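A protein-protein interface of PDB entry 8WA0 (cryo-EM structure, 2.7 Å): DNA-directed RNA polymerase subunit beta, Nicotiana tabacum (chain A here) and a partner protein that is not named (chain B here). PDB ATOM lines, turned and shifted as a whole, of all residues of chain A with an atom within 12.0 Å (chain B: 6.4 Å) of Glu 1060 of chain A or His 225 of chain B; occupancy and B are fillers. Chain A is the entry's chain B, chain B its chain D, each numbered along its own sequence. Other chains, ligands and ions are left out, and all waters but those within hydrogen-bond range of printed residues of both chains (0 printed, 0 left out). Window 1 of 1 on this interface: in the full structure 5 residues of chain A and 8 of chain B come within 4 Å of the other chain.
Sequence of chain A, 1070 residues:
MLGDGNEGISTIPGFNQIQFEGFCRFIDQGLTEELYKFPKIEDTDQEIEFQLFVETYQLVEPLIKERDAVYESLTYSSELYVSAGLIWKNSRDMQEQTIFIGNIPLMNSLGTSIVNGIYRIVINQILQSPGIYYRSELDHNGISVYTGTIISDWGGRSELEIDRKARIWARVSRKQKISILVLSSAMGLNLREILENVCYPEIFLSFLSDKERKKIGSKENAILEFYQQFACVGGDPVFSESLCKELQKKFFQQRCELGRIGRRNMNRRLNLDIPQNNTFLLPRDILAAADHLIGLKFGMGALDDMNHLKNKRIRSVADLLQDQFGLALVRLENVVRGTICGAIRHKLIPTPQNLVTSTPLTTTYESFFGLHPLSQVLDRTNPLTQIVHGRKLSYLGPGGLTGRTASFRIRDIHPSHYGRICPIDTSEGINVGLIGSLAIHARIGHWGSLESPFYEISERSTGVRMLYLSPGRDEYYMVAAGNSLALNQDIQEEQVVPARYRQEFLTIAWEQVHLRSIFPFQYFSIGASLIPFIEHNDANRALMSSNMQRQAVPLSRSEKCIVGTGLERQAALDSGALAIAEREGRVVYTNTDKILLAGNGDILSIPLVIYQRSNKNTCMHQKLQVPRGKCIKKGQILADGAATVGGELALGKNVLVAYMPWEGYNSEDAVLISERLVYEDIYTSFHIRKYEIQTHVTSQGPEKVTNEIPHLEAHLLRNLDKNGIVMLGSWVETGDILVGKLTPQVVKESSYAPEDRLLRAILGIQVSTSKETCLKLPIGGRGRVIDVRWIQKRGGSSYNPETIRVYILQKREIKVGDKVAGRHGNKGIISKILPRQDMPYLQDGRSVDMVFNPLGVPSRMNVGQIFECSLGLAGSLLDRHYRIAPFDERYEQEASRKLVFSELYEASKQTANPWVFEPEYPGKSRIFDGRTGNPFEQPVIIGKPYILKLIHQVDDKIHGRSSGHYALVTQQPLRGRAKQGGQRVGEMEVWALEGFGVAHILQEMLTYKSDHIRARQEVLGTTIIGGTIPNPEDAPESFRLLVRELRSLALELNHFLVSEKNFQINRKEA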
ATOM      1  N   PHE A1056       7.756 -17.340 -27.492  1.00  0.00           N
ATOM      2  CA  PHE A1056       8.512 -17.050 -26.302  1.00  0.00           C
ATOM      3  C   PHE A1056       8.961 -18.333 -25.662  1.00  0.00           C
ATOM      4  O   PHE A1056       8.268 -19.333 -25.759  1.00  0.00           O
ATOM      5  CB  PHE A1056       7.647 -16.347 -25.276  1.00  0.00           C
ATOM      6  CG  PHE A1056       7.039 -15.065 -25.736  1.00  0.00           C
ATOM      7  CD1 PHE A1056       7.759 -13.894 -25.698  1.00  0.00           C
ATOM      8  CD2 PHE A1056       5.721 -15.023 -26.144  1.00  0.00           C
ATOM      9  CE1 PHE A1056       7.192 -12.705 -26.098  1.00  0.00           C
ATOM     10  CE2 PHE A1056       5.146 -13.840 -26.544  1.00  0.00           C
ATOM     11  CZ  PHE A1056       5.883 -12.677 -26.522  1.00  0.00           C
ATOM     12  N   LEU A1057      10.109 -18.328 -25.005  1.00  0.00           N
ATOM     13  CA  LEU A1057      10.541 -19.494 -24.262  1.00  0.00           C
ATOM     14  C   LEU A1057      10.772 -19.086 -22.828  1.00  0.00           C
ATOM     15  O   LEU A1057      11.426 -18.090 -22.570  1.00  0.00           O
ATOM     16  CB  LEU A1057      11.795 -20.111 -24.861  1.00  0.00           C
ATOM     17  CG  LEU A1057      13.028 -19.259 -25.137  1.00  0.00           C
ATOM     18  CD1 LEU A1057      14.274 -20.097 -24.910  1.00  0.00           C
ATOM     19  CD2 LEU A1057      12.998 -18.756 -26.568  1.00  0.00           C
ATOM     20  N   VAL A1058      10.224 -19.840 -21.888  1.00  0.00           N
ATOM     21  CA  VAL A1058      10.370 -19.504 -20.488  1.00  0.00           C
ATOM     22  C   VAL A1058      11.391 -20.418 -19.874  1.00  0.00           C
ATOM     23  O   VAL A1058      11.267 -21.629 -19.956  1.00  0.00           O
ATOM     24  CB  VAL A1058       9.056 -19.686 -19.732  1.00  0.00           C
ATOM     25  CG1 VAL A1058       9.197 -19.198 -18.302  1.00  0.00           C
ATOM     26  CG2 VAL A1058       7.931 -18.957 -20.444  1.00  0.00           C
ATOM     27  N   SER A1059      12.415 -19.850 -19.265  1.00  0.00           N
ATOM     28  CA  SER A1059      13.468 -20.665 -18.713  1.00  0.00           C
ATOM     29  C   SER A1059      13.007 -21.365 -17.477  1.00  0.00           C
ATOM     30  O   SER A1059      12.438 -20.756 -16.591  1.00  0.00           O
ATOM     31  CB  SER A1059      14.666 -19.810 -18.372  1.00  0.00           C
ATOM     32  OG  SER A1059      15.576 -20.527 -17.558  1.00  0.00           O
ATOM     33  N   GLU A1060      13.250 -22.659 -17.411  1.00  0.00           N
ATOM     34  CA  GLU A1060      12.862 -23.421 -16.244  1.00  0.00           C
ATOM     35  C   GLU A1060      13.638 -23.025 -15.015  1.00  0.00           C
ATOM     36  O   GLU A1060      13.077 -22.951 -13.934  1.00  0.00           O
ATOM     37  CB  GLU A1060      12.955 -24.930 -16.497  1.00  0.00           C
ATOM     38  CG  GLU A1060      14.339 -25.480 -16.813  1.00  0.00           C
ATOM     39  CD  GLU A1060      14.800 -25.174 -18.225  1.00  0.00           C
ATOM     40  OE1 GLU A1060      13.940 -24.927 -19.096  1.00  0.00           O
ATOM     41  OE2 GLU A1060      16.025 -25.181 -18.462  1.00  0.00           O
ATOM     42  N   LYS A1061      14.931 -22.797 -15.159  1.00  0.00           N
ATOM     43  CA  LYS A1061      15.738 -22.494 -14.001  1.00  0.00           C
ATOM     44  C   LYS A1061      15.457 -21.181 -13.287  1.00  0.00           C
ATOM     45  O   LYS A1061      15.366 -21.165 -12.069  1.00  0.00           O
ATOM     46  CB  LYS A1061      17.203 -22.592 -14.374  1.00  0.00           C
ATOM     47  CG  LYS A1061      17.649 -24.009 -14.674  1.00  0.00           C
ATOM     48  CD  LYS A1061      19.153 -24.089 -14.853  1.00  0.00           C
ATOM     49  CE  LYS A1061      19.603 -25.533 -14.992  1.00  0.00           C
ATOM     50  NZ  LYS A1061      21.085 -25.647 -15.047  1.00  0.00           N
ATOM     51  N   ASN A1062      15.296 -20.087 -14.017  1.00  0.00           N
ATOM     52  CA  ASN A1062      15.119 -18.793 -13.369  1.00  0.00           C
ATOM     53  C   ASN A1062      13.807 -18.110 -13.645  1.00  0.00           C
ATOM     54  O   ASN A1062      13.567 -17.046 -13.096  1.00  0.00           O
ATOM     55  CB  ASN A1062      16.269 -17.876 -13.745  1.00  0.00           C
ATOM     56  CG  ASN A1062      16.457 -17.740 -15.242  1.00  0.00           C
ATOM     57  OD1 ASN A1062      15.521 -17.890 -16.018  1.00  0.00           O
ATOM     58  ND2 ASN A1062      17.679 -17.434 -15.653  1.00  0.00           N
ATOM     59  N   PHE A1063      12.990 -18.679 -14.519  1.00  0.00           N
ATOM     60  CA  PHE A1063      11.661 -18.141 -14.855  1.00  0.00           C
ATOM     61  C   PHE A1063      11.603 -16.943 -15.795  1.00  0.00           C
ATOM     62  O   PHE A1063      10.545 -16.357 -15.965  1.00  0.00           O
ATOM     63  CB  PHE A1063      10.786 -17.912 -13.617  1.00  0.00           C
ATOM     64  CG  PHE A1063      10.773 -19.065 -12.654  1.00  0.00           C
ATOM     65  CD1 PHE A1063      10.650 -20.365 -13.105  1.00  0.00           C
ATOM     66  CD2 PHE A1063      10.874 -18.841 -11.295  1.00  0.00           C
ATOM     67  CE1 PHE A1063      10.644 -21.420 -12.217  1.00  0.00           C
ATOM     68  CE2 PHE A1063      10.864 -19.890 -10.402  1.00  0.00           C
ATOM     69  CZ  PHE A1063      10.749 -21.181 -10.864  1.00  0.00           C
ATOM     70  N   GLN A1064      12.718 -16.581 -16.411  1.00  0.00           N
ATOM     71  CA  GLN A1064      12.726 -15.479 -17.376  1.00  0.00           C
ATOM     72  C   GLN A1064      12.053 -15.802 -18.707  1.00  0.00           C
ATOM     73  O   GLN A1064      12.178 -16.913 -19.199  1.00  0.00           O
ATOM     74  CB  GLN A1064      14.152 -15.027 -17.632  1.00  0.00           C
ATOM     75  CG  GLN A1064      14.850 -14.500 -16.397  1.00  0.00           C
ATOM     76  CD  GLN A1064      16.242 -13.999 -16.701  1.00  0.00           C
ATOM     77  OE1 GLN A1064      17.030 -13.727 -15.796  1.00  0.00           O
ATOM     78  NE2 GLN A1064      16.557 -13.876 -17.984  1.00  0.00           N
ATOM     79  N   ILE A1065      11.370 -14.833 -19.309  1.00  0.00           N
ATOM     80  CA  ILE A1065      10.699 -15.052 -20.583  1.00  0.00           C
ATOM     81  C   ILE A1065      11.476 -14.382 -21.686  1.00  0.00           C
ATOM     82  O   ILE A1065      11.726 -13.190 -21.616  1.00  0.00           O
ATOM     83  CB  ILE A1065       9.294 -14.457 -20.575  1.00  0.00           C
ATOM     84  CG1 ILE A1065       8.509 -14.963 -19.371  1.00  0.00           C
ATOM     85  CG2 ILE A1065       8.560 -14.797 -21.861  1.00  0.00           C
ATOM     86  CD1 ILE A1065       7.084 -14.461 -19.335  1.00  0.00           C
ATOM     87  N   ASN A1066      11.864 -15.125 -22.710  1.00  0.00           N
ATOM     88  CA  ASN A1066      12.692 -14.567 -23.769  1.00  0.00           C
ATOM     89  C   ASN A1066      11.997 -14.667 -25.093  1.00  0.00           C
ATOM     90  O   ASN A1066      11.482 -15.716 -25.434  1.00  0.00           O
ATOM     91  CB  ASN A1066      13.992 -15.343 -23.869  1.00  0.00           C
ATOM     92  CG  ASN A1066      14.585 -15.669 -22.514  1.00  0.00           C
ATOM     93  OD1 ASN A1066      14.564 -14.847 -21.599  1.00  0.00           O
ATOM     94  ND2 ASN A1066      15.127 -16.872 -22.381  1.00  0.00           N
ATOM     95  N   LYS A1068      11.969 -15.083 -28.888  1.00  0.00           N
ATOM     96  CA  LYS A1068      12.753 -15.406 -30.064  1.00  0.00           C
ATOM     97  C   LYS A1068      12.270 -14.563 -31.218  1.00  0.00           C
ATOM     98  O   LYS A1068      11.095 -14.231 -31.294  1.00  0.00           O
ATOM     99  CB  LYS A1068      12.661 -16.881 -30.405  1.00  0.00           C
ATOM    100  CG  LYS A1068      13.876 -17.677 -29.968  1.00  0.00           C
ATOM    101  CD  LYS A1068      13.763 -19.139 -30.363  1.00  0.00           C
ATOM    102  CE  LYS A1068      15.001 -19.906 -29.929  1.00  0.00           C
ATOM    103  NZ  LYS A1068      14.924 -21.355 -30.263  1.00  0.00           N
ATOM    104  N   ASP B 219      18.459 -23.320  -0.182  1.00  0.00           N
ATOM    105  CA  ASP B 219      18.390 -22.507  -1.364  1.00  0.00           C
ATOM    106  C   ASP B 219      17.000 -22.063  -1.672  1.00  0.00           C
ATOM    107  O   ASP B 219      16.786 -20.933  -2.053  1.00  0.00           O
ATOM    108  CB  ASP B 219      19.001 -23.239  -2.522  1.00  0.00           C
ATOM    109  CG  ASP B 219      20.490 -23.309  -2.440  1.00  0.00           C
ATOM    110  OD1 ASP B 219      21.066 -22.691  -1.527  1.00  0.00           O
ATOM    111  OD2 ASP B 219      21.092 -23.980  -3.293  1.00  0.00           O
ATOM    112  N   CYS B 220      16.046 -22.930  -1.510  1.00  0.00           N
ATOM    113  CA  CYS B 220      14.690 -22.588  -1.729  1.00  0.00           C
ATOM    114  C   CYS B 220      14.162 -21.589  -0.769  1.00  0.00           C
ATOM    115  O   CYS B 220      13.371 -20.741  -1.158  1.00  0.00           O
ATOM    116  CB  CYS B 220      13.853 -23.819  -1.839  1.00  0.00           C
ATOM    117  SG  CYS B 220      14.260 -24.735  -3.335  1.00  0.00           S
ATOM    118  N   GLY B 223      15.470 -18.380  -2.014  1.00  0.00           N
ATOM    119  CA  GLY B 223      14.850 -18.103  -3.287  1.00  0.00           C
ATOM    120  C   GLY B 223      15.506 -18.596  -4.555  1.00  0.00           C
ATOM    121  O   GLY B 223      14.997 -18.324  -5.622  1.00  0.00           O
ATOM    122  N   ASP B 224      16.606 -19.319  -4.472  1.00  0.00           N
ATOM    123  CA  ASP B 224      17.318 -19.728  -5.675  1.00  0.00           C
ATOM    124  C   ASP B 224      16.853 -21.000  -6.293  1.00  0.00           C
ATOM    125  O   ASP B 224      17.295 -22.060  -5.912  1.00  0.00           O
ATOM    126  CB  ASP B 224      18.785 -19.877  -5.375  1.00  0.00           C
ATOM    127  CG  ASP B 224      19.655 -19.728  -6.603  1.00  0.00           C
ATOM    128  OD1 ASP B 224      19.118 -19.547  -7.716  1.00  0.00           O
ATOM    129  OD2 ASP B 224      20.892 -19.783  -6.452  1.00  0.00           O
ATOM    130  N   HIS B 225      15.975 -20.911  -7.261  1.00  0.00           N
ATOM    131  CA  HIS B 225      15.540 -22.071  -7.969  1.00  0.00           C
ATOM    132  C   HIS B 225      16.621 -22.672  -8.800  1.00  0.00           C
ATOM    133  O   HIS B 225      16.695 -23.882  -8.926  1.00  0.00           O
ATOM    134  CB  HIS B 225      14.300 -21.771  -8.770  1.00  0.00           C
ATOM    135  CG  HIS B 225      13.577 -22.976  -9.264  1.00  0.00           C
ATOM    136  ND1 HIS B 225      13.753 -23.477 -10.532  1.00  0.00           N
ATOM    137  CD2 HIS B 225      12.656 -23.764  -8.671  1.00  0.00           C
ATOM    138  CE1 HIS B 225      12.982 -24.535 -10.695  1.00  0.00           C
ATOM    139  NE2 HIS B 225      12.308 -24.731  -9.579  1.00  0.00           N
ATOM    140  N   SER B 226      17.472 -21.875  -9.379  1.00  0.00           N
ATOM    141  CA  SER B 226      18.424 -22.437 -10.288  1.00  0.00           C
ATOM    142  C   SER B 226      19.373 -23.402  -9.710  1.00  0.00           C
ATOM    143  O   SER B 226      19.565 -24.486 -10.244  1.00  0.00           O
ATOM    144  CB  SER B 226      19.232 -21.350 -10.922  1.00  0.00           C
ATOM    145  OG  SER B 226      18.400 -20.460 -11.636  1.00  0.00           O
ATOM    146  N   ASN B 227      19.947 -23.054  -8.592  1.00  0.00           N
ATOM    147  CA  ASN B 227      20.892 -23.911  -7.965  1.00  0.00           C
ATOM    148  C   ASN B 227      20.228 -25.160  -7.470  1.00  0.00           C
ATOM    149  O   ASN B 227      20.784 -26.235  -7.569  1.00  0.00           O
ATOM    150  CB  ASN B 227      21.639 -23.153  -6.907  1.00  0.00           C
ATOM    151  CG  ASN B 227      22.864 -22.470  -7.447  1.00  0.00           C
ATOM    152  OD1 ASN B 227      23.410 -21.564  -6.823  1.00  0.00           O
ATOM    153  ND2 ASN B 227      23.310 -22.903  -8.616  1.00  0.00           N
ATOM    154  N   ALA B 228      19.023 -25.039  -6.965  1.00  0.00           N
ATOM    155  CA  ALA B 228      18.326 -26.170  -6.427  1.00  0.00           C
ATOM    156  C   ALA B 228      18.011 -27.261  -7.387  1.00  0.00           C
ATOM    157  O   ALA B 228      18.226 -28.416  -7.085  1.00  0.00           O
ATOM    158  CB  ALA B 228      17.058 -25.687  -5.811  1.00  0.00           C
ATOM    159  N   LEU B 229      17.512 -26.922  -8.559  1.00  0.00           N
ATOM    160  CA  LEU B 229      17.240 -27.916  -9.559  1.00  0.00           C
ATOM    161  C   LEU B 229      18.512 -28.551 -10.045  1.00  0.00           C
ATOM    162  O   LEU B 229      18.529 -29.741 -10.285  1.00  0.00           O
ATOM    163  CB  LEU B 229      16.307 -27.422 -10.658  1.00  0.00           C
ATOM    164  CG  LEU B 229      15.657 -28.341 -11.667  1.00  0.00           C
ATOM    165  CD1 LEU B 229      14.728 -29.321 -10.978  1.00  0.00           C
ATOM    166  CD2 LEU B 229      14.892 -27.496 -12.665  1.00  0.00           C
ATOM    167  N   THR B 230      19.591 -27.816 -10.176  1.00  0.00           N
ATOM    168  CA  THR B 230      20.781 -28.462 -10.620  1.00  0.00           C
ATOM    169  C   THR B 230      21.204 -29.530  -9.629  1.00  0.00           C
ATOM    170  O   THR B 230      21.597 -30.612 -10.030  1.00  0.00           O
ATOM    171  CB  THR B 230      21.848 -27.441 -10.902  1.00  0.00           C
ATOM    172  OG1 THR B 230      21.240 -26.302 -11.509  1.00  0.00           O
ATOM    173  CG2 THR B 230      22.890 -28.009 -11.838  1.00  0.00           C
ATOM    174  N   TYR B 233      18.946 -32.679  -9.788  1.00  0.00           N
ATOM    175  CA  TYR B 233      19.215 -33.494 -10.929  1.00  0.00           C
ATOM    176  C   TYR B 233      20.408 -34.330 -10.670  1.00  0.00           C
ATOM    177  O   TYR B 233      20.431 -35.497 -11.033  1.00  0.00           O
ATOM    178  CB  TYR B 233      19.359 -32.687 -12.175  1.00  0.00           C
ATOM    179  CG  TYR B 233      18.075 -32.331 -12.846  1.00  0.00           C
ATOM    180  CD1 TYR B 233      17.022 -33.208 -12.864  1.00  0.00           C
ATOM    181  CD2 TYR B 233      17.930 -31.128 -13.492  1.00  0.00           C
ATOM    182  CE1 TYR B 233      15.845 -32.886 -13.493  1.00  0.00           C
ATOM    183  CE2 TYR B 233      16.757 -30.797 -14.119  1.00  0.00           C
ATOM    184  CZ  TYR B 233      15.720 -31.681 -14.112  1.00  0.00           C
ATOM    185  OH  TYR B 233      14.551 -31.350 -14.740  1.00  0.00           O
ATOM    186  N   CYS B 249       9.701 -28.216  -1.631  1.00  0.00           N
ATOM    187  CA  CYS B 249      10.589 -27.097  -1.553  1.00  0.00           C
ATOM    188  C   CYS B 249      10.707 -26.381  -2.875  1.00  0.00           C
ATOM    189  O   CYS B 249      10.656 -25.167  -2.926  1.00  0.00           O
ATOM    190  CB  CYS B 249      11.931 -27.608  -1.092  1.00  0.00           C
ATOM    191  SG  CYS B 249      11.936 -28.267   0.573  1.00  0.00           S
ATOM    192  N   LEU B 250      10.818 -27.114  -3.952  1.00  0.00           N
ATOM    193  CA  LEU B 250      10.946 -26.532  -5.257  1.00  0.00           C
ATOM    194  C   LEU B 250       9.728 -25.760  -5.623  1.00  0.00           C
ATOM    195  O   LEU B 250       9.834 -24.693  -6.199  1.00  0.00           O
ATOM    196  CB  LEU B 250      11.293 -27.604  -6.285  1.00  0.00           C
ATOM    197  CG  LEU B 250      12.726 -27.786  -6.772  1.00  0.00           C
ATOM    198  CD1 LEU B 250      13.705 -27.906  -5.624  1.00  0.00           C
ATOM    199  CD2 LEU B 250      12.811 -29.005  -7.666  1.00  0.00           C
ATOM    200  N   LEU B 251       8.572 -26.259  -5.281  1.00  0.00           N
ATOM    201  CA  LEU B 251       7.319 -25.610  -5.588  1.00  0.00           C
ATOM    202  C   LEU B 251       7.147 -24.297  -4.913  1.00  0.00           C
ATOM    203  O   LEU B 251       6.407 -23.470  -5.384  1.00  0.00           O
ATOM    204  CB  LEU B 251       6.132 -26.536  -5.332  1.00  0.00           C
ATOM    205  CG  LEU B 251       5.655 -27.627  -6.264  1.00  0.00           C
ATOM    206  CD1 LEU B 251       5.089 -28.739  -5.415  1.00  0.00           C
ATOM    207  CD2 LEU B 251       4.593 -27.093  -7.198  1.00  0.00           C
ATOM    208  N   VAL B 253       9.331 -21.838  -4.492  1.00  0.00           N
ATOM    209  CA  VAL B 253       9.831 -20.823  -5.351  1.00  0.00           C
ATOM    210  C   VAL B 253       9.013 -20.687  -6.611  1.00  0.00           C
ATOM    211  O   VAL B 253       8.861 -19.604  -7.130  1.00  0.00           O
ATOM    212  CB  VAL B 253      11.282 -21.019  -5.593  1.00  0.00           C
ATOM    213  CG1 VAL B 253      11.896 -19.776  -6.207  1.00  0.00           C
ATOM    214  CG2 VAL B 253      11.971 -21.355  -4.292  1.00  0.00           C
ATOM    215  N   GLN B 254       8.511 -21.771  -7.144  1.00  0.00           N
ATOM    216  CA  GLN B 254       7.692 -21.764  -8.350  1.00  0.00           C
ATOM    217  C   GLN B 254       6.354 -21.104  -8.296  1.00  0.00           C
ATOM    218  O   GLN B 254       5.940 -20.499  -9.264  1.00  0.00           O
ATOM    219  CB  GLN B 254       7.532 -23.166  -8.910  1.00  0.00           C
ATOM    220  CG  GLN B 254       8.790 -23.851  -9.376  1.00  0.00           C
ATOM    221  CD  GLN B 254       8.513 -25.259  -9.829  1.00  0.00           C
ATOM    222  OE1 GLN B 254       7.370 -25.671  -9.910  1.00  0.00           O
ATOM    223  NE2 GLN B 254       9.552 -25.998 -10.128  1.00  0.00           N
ATOM    224  N   ILE B 262       3.851 -23.549 -14.729  1.00  0.00           N
ATOM    225  CA  ILE B 262       5.090 -24.184 -14.322  1.00  0.00           C
ATOM    226  C   ILE B 262       4.890 -25.056 -13.093  1.00  0.00           C
ATOM    227  O   ILE B 262       5.510 -26.103 -12.997  1.00  0.00           O
ATOM    228  CB  ILE B 262       6.228 -23.185 -14.125  1.00  0.00           C
ATOM    229  CG1 ILE B 262       5.893 -22.200 -13.020  1.00  0.00           C
ATOM    230  CG2 ILE B 262       6.504 -22.440 -15.419  1.00  0.00           C
ATOM    231  CD1 ILE B 262       7.118 -21.558 -12.436  1.00  0.00           C
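A ring nitrogen (ND1) of His 225 of chain B sits at hydrogen-bond distance from the backbone carbonyl oxygen (O) of Lys 1061 of chain A.
OG of Ser 226 of chain B lies within hydrogen-bond range of O of Lys 1061 of chain A (3.1 Å).
Of chain B, only His 225 (3.5 Å) comes within 4 Å of Glu 1060 of chain A.
Printed residues of chain B within 4 Å of Lys 1061 of chain A: His 225 (3.2 Å), Ser 226 (3.1 Å) and Thr 230 (3.6 Å).
Of the printed residues of chain B, Asn 1062 of chain A touches Ser 226.
Of the printed residues of chain B, Phe 1063 of chain A touches His 225 (3.7 Å), Val 253 (3.8 Å), Gln 254 (3.6 Å) and Ile 262 (3.5 Å).
No residue of chain A comes within 4 Å of Cys 220 of chain B.
Asp 224 of chain B touches none of the printed residues of chain A.
His 225 of chain B touches three residues of chain A.
Ser 226 of chain B touches two residues of chain A.
No residue of chain A comes within 4 Å of Ala 228 of chain B.
No residue of chain A comes within 4 Å of Leu 229 of chain B.
No residue of chain A comes within 4 Å of Leu 250 of chain B.
Val 253 of chain B touches just one residue of chain A: Phe 1063 (3.8 Å).
Of chain A, only Phe 1063 comes within 4 Å of Gln 254 of chain B.
Printed residues of chain A within 4 Å of Ile 262 of chain B: Phe 1063 (3.5 Å).
The nearest residue of chain B that does not touch Glu 1060 of chain A is Leu 229 of chain B (4.6 Å).
The nearest residue of chain A that does not touch His 225 of chain B is Asn 1062 of chain A (5.1 Å).
The nearest printed residue of chain B that does not touch Asn 1062 of chain A is His 225 of chain B (5.1 Å).
Of the 12 printed residues of chain A, 4 touch a printed residue of chain B.
Along chain A the printed residues that touch a printed residue of chain B span positions 1060 to 1063.
Hydrophobic or aromatic side chains of chain B that line the printed part of chain A: His 225 and Ile 262.
Along chain B the printed residues that touch a printed residue of chain A span positions 225 to 262.
Among the printed residues, no Asp or Glu carboxylate lies within 4 Å of a Lys or Arg side-chain nitrogen of the other chain.
Glu 1060 of chain A touches His 225 of chain B (O to ND1, 3.5 Å).
OG1 of Thr 230 of chain B touches NZ of Lys 1061 of chain A, at 3.6 Å.
Asn 1062 of chain A touches Ser 226 of chain B (N to OG, 3.9 Å).
His 225 of chain B touches Phe 1063 of chain A.
Phe 1063 of chain A touches Val 253 of chain B.
Gln 254 of chain B touches Phe 1063 of chain A.
Ile 262 of chain B touches Phe 1063 of chain A (CD1 to CE1, 3.5 Å).
The side-chain hydroxyl (OG) of Ser 1059 of chain A sits close to the backbone NH (N) of Lys 1061 of chain A, 3.4 Å away.
The side-chain hydroxyl (OG) of Ser 1059 of chain A sits at hydrogen-bond distance from the side-chain amide oxygen (OD1) of Asn 1062 of chain A (3.1 Å).
OD1 of Asn 1062 of chain A lies within hydrogen-bond range of N of Gln 1064 of chain A, at 3.1 Å.
The side-chain carboxylate of Asp 224 of chain B sits close to the backbone NH of Ser 226 of chain B, at 3.3 Å.
The side-chain amide nitrogen (NE2) of Gln 254 of chain B is in hydrogen-bond range of a ring nitrogen (NE2) of His 225 of chain B.
The side-chain hydroxyl of Thr 230 of chain B is in hydrogen-bond range of the backbone carbonyl oxygen of Ser 226 of chain B.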
